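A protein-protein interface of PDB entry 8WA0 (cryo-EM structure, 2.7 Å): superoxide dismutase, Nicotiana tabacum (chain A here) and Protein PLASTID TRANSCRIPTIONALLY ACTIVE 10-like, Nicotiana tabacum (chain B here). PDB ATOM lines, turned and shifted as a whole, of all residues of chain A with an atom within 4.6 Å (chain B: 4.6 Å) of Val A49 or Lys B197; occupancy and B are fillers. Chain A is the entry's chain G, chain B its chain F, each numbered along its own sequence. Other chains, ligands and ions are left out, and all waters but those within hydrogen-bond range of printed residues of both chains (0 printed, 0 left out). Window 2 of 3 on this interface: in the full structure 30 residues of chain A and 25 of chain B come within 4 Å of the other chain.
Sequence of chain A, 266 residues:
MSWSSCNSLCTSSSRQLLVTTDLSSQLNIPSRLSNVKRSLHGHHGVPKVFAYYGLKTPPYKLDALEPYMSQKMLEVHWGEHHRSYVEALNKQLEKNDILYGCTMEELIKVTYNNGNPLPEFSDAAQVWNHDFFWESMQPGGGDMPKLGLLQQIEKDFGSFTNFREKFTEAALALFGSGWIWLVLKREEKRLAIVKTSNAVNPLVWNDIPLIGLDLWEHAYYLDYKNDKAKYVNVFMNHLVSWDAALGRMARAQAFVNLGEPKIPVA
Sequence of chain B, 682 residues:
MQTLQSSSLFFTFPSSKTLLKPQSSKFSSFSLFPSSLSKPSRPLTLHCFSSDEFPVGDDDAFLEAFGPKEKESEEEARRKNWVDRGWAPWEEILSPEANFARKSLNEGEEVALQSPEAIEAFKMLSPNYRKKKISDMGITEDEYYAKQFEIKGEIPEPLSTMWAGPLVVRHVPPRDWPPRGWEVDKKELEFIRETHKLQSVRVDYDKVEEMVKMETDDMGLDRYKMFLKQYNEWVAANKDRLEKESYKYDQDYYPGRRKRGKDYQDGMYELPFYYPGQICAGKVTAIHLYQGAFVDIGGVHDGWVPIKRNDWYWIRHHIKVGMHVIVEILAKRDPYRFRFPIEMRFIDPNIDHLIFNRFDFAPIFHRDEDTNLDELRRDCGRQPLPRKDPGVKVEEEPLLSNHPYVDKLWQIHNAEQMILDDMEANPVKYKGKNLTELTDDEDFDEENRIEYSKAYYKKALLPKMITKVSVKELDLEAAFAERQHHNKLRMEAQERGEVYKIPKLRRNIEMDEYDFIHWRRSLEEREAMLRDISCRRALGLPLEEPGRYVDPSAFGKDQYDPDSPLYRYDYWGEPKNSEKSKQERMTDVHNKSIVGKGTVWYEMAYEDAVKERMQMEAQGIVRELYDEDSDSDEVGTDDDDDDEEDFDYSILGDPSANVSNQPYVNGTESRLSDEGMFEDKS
The backbone NH (N) of Phe A50 sits close to the side-chain amino group (NZ) of Lys B197, at 2.9 Å.
The side-chain hydroxyl (OG) of Ser B200 is in hydrogen-bond range of the backbone carbonyl oxygen (O) of Lys B197 (3.1 Å).
The backbone NH of Phe A50 lies within hydrogen-bond range of the side-chain hydroxyl of Tyr A100, 3.5 Å away.
Val A49 touches Arg B193.
Val A49 touches Lys B197.
CB of His B196 touches O of Phe A50, at 3.7 Å.
CE2 of Tyr A100 touches NH1 of Arg B193, 3.2 Å away.
Tyr A100 touches His B196.
Printed residues of chain B within 4 Å of Val A49: Arg B193 and Lys B197.
Of the printed residues of chain B, Phe A50 touches His B196 (3.7 Å) and Lys B197 (2.9 Å).
Ala A51 touches none of the printed residues of chain B.
Of the printed residues of chain B, Tyr A100 touches Arg B193 (3.2 Å) and His B196 (3.2 Å).
Printed residues of chain A within 4 Å of Arg B193: Val A49 and Tyr A100.
Of the printed residues of chain A, His B196 touches Phe A50 (3.7 Å) and Tyr A100 (3.2 Å).
Lys B197 touches two residues of chain A.
The nearest printed residue of chain A that does not touch Lys B197 is Ala A51 (5.2 Å).
Of the 9 printed residues of chain B, 3 touch a printed residue of chain A.
Printed residues of chain B that touch a printed residue of chain A: Arg B193, His B196 and Lys B197.
Hydrophobic or aromatic side chains of chain B within 4 Å of the printed part of chain A: His B196.
Printed residues of chain A that touch a printed residue of chain B: Val A49, Phe A50 and Tyr A100.
Hydrophobic or aromatic side chains of chain A that line the printed part of chain B: Phe A50 and Tyr A100.
Among the printed residues, 6 pairs touch across the chains.
Among the printed residues, no Asp or Glu carboxylate lies within 4 Å of a Lys or Arg side-chain nitrogen of the other chain.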
ATOM      1  N   VAL A  49     -26.400  -8.156 -29.964  1.00  0.00           N
ATOM      2  CA  VAL A  49     -27.583  -7.830 -30.697  1.00  0.00           C
ATOM      3  C   VAL A  49     -27.996  -6.453 -30.333  1.00  0.00           C
ATOM      4  O   VAL A  49     -28.757  -5.826 -31.053  1.00  0.00           O
ATOM      5  CB  VAL A  49     -28.723  -8.769 -30.344  1.00  0.00           C
ATOM      6  N   PHE A  50     -27.517  -5.960 -29.211  1.00  0.00           N
ATOM      7  CA  PHE A  50     -27.965  -4.666 -28.765  1.00  0.00           C
ATOM      8  C   PHE A  50     -26.933  -3.691 -28.341  1.00  0.00           C
ATOM      9  O   PHE A  50     -26.102  -3.987 -27.504  1.00  0.00           O
ATOM     10  CB  PHE A  50     -28.979  -4.820 -27.655  1.00  0.00           C
ATOM     11  N   ALA A  51     -27.020  -2.500 -28.884  1.00  0.00           N
ATOM     12  CA  ALA A  51     -26.048  -1.464 -28.603  1.00  0.00           C
ATOM     13  C   ALA A  51     -26.920  -0.275 -28.347  1.00  0.00           C
ATOM     14  O   ALA A  51     -28.077  -0.293 -28.767  1.00  0.00           O
ATOM     15  CB  ALA A  51     -25.150  -1.224 -29.804  1.00  0.00           C
ATOM     16  N   ASN A  90     -33.453  -2.597 -29.469  1.00  0.00           N
ATOM     17  CA  ASN A  90     -32.477  -3.581 -29.711  1.00  0.00           C
ATOM     18  C   ASN A  90     -32.884  -4.528 -30.782  1.00  0.00           C
ATOM     19  O   ASN A  90     -32.099  -4.882 -31.638  1.00  0.00           O
ATOM     20  CB  ASN A  90     -32.276  -4.290 -28.425  1.00  0.00           C
ATOM     21  CG  ASN A  90     -31.840  -3.357 -27.319  1.00  0.00           C
ATOM     22  OD1 ASN A  90     -31.486  -2.208 -27.570  1.00  0.00           O
ATOM     23  ND2 ASN A  90     -31.844  -3.851 -26.089  1.00  0.00           N
ATOM     24  N   LEU A  93     -32.820  -3.108 -34.093  1.00  0.00           N
ATOM     25  CA  LEU A  93     -31.445  -3.023 -34.556  1.00  0.00           C
ATOM     26  C   LEU A  93     -30.872  -4.266 -35.085  1.00  0.00           C
ATOM     27  O   LEU A  93     -30.031  -4.219 -35.967  1.00  0.00           O
ATOM     28  CB  LEU A  93     -30.508  -2.470 -33.486  1.00  0.00           C
ATOM     29  N   GLU A  94     -31.286  -5.391 -34.577  1.00  0.00           N
ATOM     30  CA  GLU A  94     -30.647  -6.616 -34.958  1.00  0.00           C
ATOM     31  C   GLU A  94     -30.733  -6.816 -36.435  1.00  0.00           C
ATOM     32  O   GLU A  94     -29.836  -7.366 -37.054  1.00  0.00           O
ATOM     33  CB  GLU A  94     -31.234  -7.783 -34.197  1.00  0.00           C
ATOM     34  CG  GLU A  94     -30.887  -9.168 -34.727  1.00  0.00           C
ATOM     35  CD  GLU A  94     -29.426  -9.545 -34.550  1.00  0.00           C
ATOM     36  OE1 GLU A  94     -28.688  -8.824 -33.848  1.00  0.00           O
ATOM     37  OE2 GLU A  94     -29.013 -10.579 -35.114  1.00  0.00           O
ATOM     38  N   TYR A 100     -26.524  -0.461 -36.748  1.00  0.00           N
ATOM     39  CA  TYR A 100     -25.959  -0.853 -35.455  1.00  0.00           C
ATOM     40  C   TYR A 100     -24.772  -0.018 -35.194  1.00  0.00           C
ATOM     41  O   TYR A 100     -24.567   0.433 -34.085  1.00  0.00           O
ATOM     42  CB  TYR A 100     -25.485  -2.294 -35.496  1.00  0.00           C
ATOM     43  CG  TYR A 100     -25.217  -2.958 -34.173  1.00  0.00           C
ATOM     44  CD1 TYR A 100     -26.237  -3.574 -33.475  1.00  0.00           C
ATOM     45  CD2 TYR A 100     -23.941  -3.009 -33.645  1.00  0.00           C
ATOM     46  CE1 TYR A 100     -25.999  -4.199 -32.272  1.00  0.00           C
ATOM     47  CE2 TYR A 100     -23.695  -3.631 -32.440  1.00  0.00           C
ATOM     48  CZ  TYR A 100     -24.729  -4.228 -31.762  1.00  0.00           C
ATOM     49  OH  TYR A 100     -24.498  -4.851 -30.562  1.00  0.00           O
ATOM     50  N   GLU B 190     -22.061 -12.910 -31.894  1.00  0.00           N
ATOM     51  CA  GLU B 190     -23.002 -12.622 -30.856  1.00  0.00           C
ATOM     52  C   GLU B 190     -22.261 -12.479 -29.588  1.00  0.00           C
ATOM     53  O   GLU B 190     -22.576 -11.636 -28.760  1.00  0.00           O
ATOM     54  CB  GLU B 190     -24.016 -13.736 -30.722  1.00  0.00           C
ATOM     55  CG  GLU B 190     -24.880 -13.937 -31.956  1.00  0.00           C
ATOM     56  CD  GLU B 190     -25.619 -12.679 -32.370  1.00  0.00           C
ATOM     57  OE1 GLU B 190     -26.236 -12.031 -31.498  1.00  0.00           O
ATOM     58  OE2 GLU B 190     -25.595 -12.346 -33.573  1.00  0.00           O
ATOM     59  N   ARG B 193     -20.671  -9.042 -29.384  1.00  0.00           N
ATOM     60  CA  ARG B 193     -21.505  -7.914 -29.160  1.00  0.00           C
ATOM     61  C   ARG B 193     -22.141  -7.856 -27.828  1.00  0.00           C
ATOM     62  O   ARG B 193     -22.888  -6.931 -27.543  1.00  0.00           O
ATOM     63  CB  ARG B 193     -22.520  -7.838 -30.247  1.00  0.00           C
ATOM     64  CG  ARG B 193     -21.916  -7.441 -31.587  1.00  0.00           C
ATOM     65  CD  ARG B 193     -22.429  -8.316 -32.719  1.00  0.00           C
ATOM     66  NE  ARG B 193     -22.110  -7.800 -34.042  1.00  0.00           N
ATOM     67  CZ  ARG B 193     -22.828  -6.885 -34.681  1.00  0.00           C
ATOM     68  NH1 ARG B 193     -23.902  -6.363 -34.115  1.00  0.00           N
ATOM     69  NH2 ARG B 193     -22.460  -6.479 -35.887  1.00  0.00           N
ATOM     70  N   GLU B 194     -21.880  -8.835 -26.994  1.00  0.00           N
ATOM     71  CA  GLU B 194     -22.396  -8.807 -25.649  1.00  0.00           C
ATOM     72  C   GLU B 194     -21.834  -7.648 -24.920  1.00  0.00           C
ATOM     73  O   GLU B 194     -22.515  -7.011 -24.137  1.00  0.00           O
ATOM     74  CB  GLU B 194     -22.034 -10.072 -24.917  1.00  0.00           C
ATOM     75  CG  GLU B 194     -22.696 -10.231 -23.558  1.00  0.00           C
ATOM     76  CD  GLU B 194     -24.187 -10.494 -23.656  1.00  0.00           C
ATOM     77  OE1 GLU B 194     -24.631 -11.055 -24.681  1.00  0.00           O
ATOM     78  OE2 GLU B 194     -24.913 -10.151 -22.701  1.00  0.00           O
ATOM     79  N   THR B 195     -20.584  -7.339 -25.172  1.00  0.00           N
ATOM     80  CA  THR B 195     -19.959  -6.271 -24.433  1.00  0.00           C
ATOM     81  C   THR B 195     -20.643  -4.974 -24.631  1.00  0.00           C
ATOM     82  O   THR B 195     -20.603  -4.124 -23.754  1.00  0.00           O
ATOM     83  CB  THR B 195     -18.525  -6.021 -24.834  1.00  0.00           C
ATOM     84  OG1 THR B 195     -18.072  -4.828 -24.208  1.00  0.00           O
ATOM     85  CG2 THR B 195     -18.406  -5.828 -26.329  1.00  0.00           C
ATOM     86  N   HIS B 196     -21.276  -4.782 -25.766  1.00  0.00           N
ATOM     87  CA  HIS B 196     -21.823  -3.502 -26.033  1.00  0.00           C
ATOM     88  C   HIS B 196     -22.809  -3.199 -24.951  1.00  0.00           C
ATOM     89  O   HIS B 196     -22.908  -2.060 -24.513  1.00  0.00           O
ATOM     90  CB  HIS B 196     -22.396  -3.451 -27.410  1.00  0.00           C
ATOM     91  CG  HIS B 196     -21.372  -3.561 -28.491  1.00  0.00           C
ATOM     92  ND1 HIS B 196     -20.080  -3.113 -28.339  1.00  0.00           N
ATOM     93  CD2 HIS B 196     -21.454  -4.055 -29.748  1.00  0.00           C
ATOM     94  CE1 HIS B 196     -19.405  -3.337 -29.451  1.00  0.00           C
ATOM     95  NE2 HIS B 196     -20.216  -3.906 -30.323  1.00  0.00           N
ATOM     96  N   LYS B 197     -23.527  -4.200 -24.487  1.00  0.00           N
ATOM     97  CA  LYS B 197     -24.500  -4.015 -23.404  1.00  0.00           C
ATOM     98  C   LYS B 197     -23.911  -3.605 -22.073  1.00  0.00           C
ATOM     99  O   LYS B 197     -24.513  -2.844 -21.331  1.00  0.00           O
ATOM    100  CB  LYS B 197     -25.338  -5.278 -23.239  1.00  0.00           C
ATOM    101  CG  LYS B 197     -25.791  -5.872 -24.561  1.00  0.00           C
ATOM    102  CD  LYS B 197     -26.393  -7.253 -24.373  1.00  0.00           C
ATOM    103  CE  LYS B 197     -26.609  -7.937 -25.712  1.00  0.00           C
ATOM    104  NZ  LYS B 197     -27.501  -7.141 -26.599  1.00  0.00           N
ATOM    105  N   LEU B 198     -22.730  -4.094 -21.770  1.00  0.00           N
ATOM    106  CA  LEU B 198     -22.129  -3.846 -20.461  1.00  0.00           C
ATOM    107  C   LEU B 198     -21.787  -2.406 -20.083  1.00  0.00           C
ATOM    108  O   LEU B 198     -21.579  -2.113 -18.917  1.00  0.00           O
ATOM    109  CB  LEU B 198     -20.904  -4.740 -20.311  1.00  0.00           C
ATOM    110  CG  LEU B 198     -21.080  -6.205 -20.706  1.00  0.00           C
ATOM    111  CD1 LEU B 198     -19.752  -6.939 -20.618  1.00  0.00           C
ATOM    112  CD2 LEU B 198     -22.128  -6.889 -19.845  1.00  0.00           C
ATOM    113  N   GLN B 199     -21.716  -1.515 -21.051  1.00  0.00           N
ATOM    114  CA  GLN B 199     -21.331  -0.123 -20.796  1.00  0.00           C
ATOM    115  C   GLN B 199     -22.326   0.726 -20.020  1.00  0.00           C
ATOM    116  O   GLN B 199     -21.996   1.833 -19.615  1.00  0.00           O
ATOM    117  CB  GLN B 199     -20.958   0.566 -22.110  1.00  0.00           C
ATOM    118  CG  GLN B 199     -19.692   1.404 -22.025  1.00  0.00           C
ATOM    119  CD  GLN B 199     -19.101   1.712 -23.386  1.00  0.00           C
ATOM    120  OE1 GLN B 199     -19.671   1.359 -24.419  1.00  0.00           O
ATOM    121  NE2 GLN B 199     -17.947   2.370 -23.395  1.00  0.00           N
ATOM    122  N   SER B 200     -23.551   0.252 -19.857  1.00  0.00           N
ATOM    123  CA  SER B 200     -24.555   0.959 -19.061  1.00  0.00           C
ATOM    124  C   SER B 200     -24.234   1.122 -17.577  1.00  0.00           C
ATOM    125  O   SER B 200     -24.621   2.106 -16.973  1.00  0.00           O
ATOM    126  CB  SER B 200     -25.895   0.258 -19.219  1.00  0.00           C
ATOM    127  OG  SER B 200     -25.744  -1.145 -19.098  1.00  0.00           O
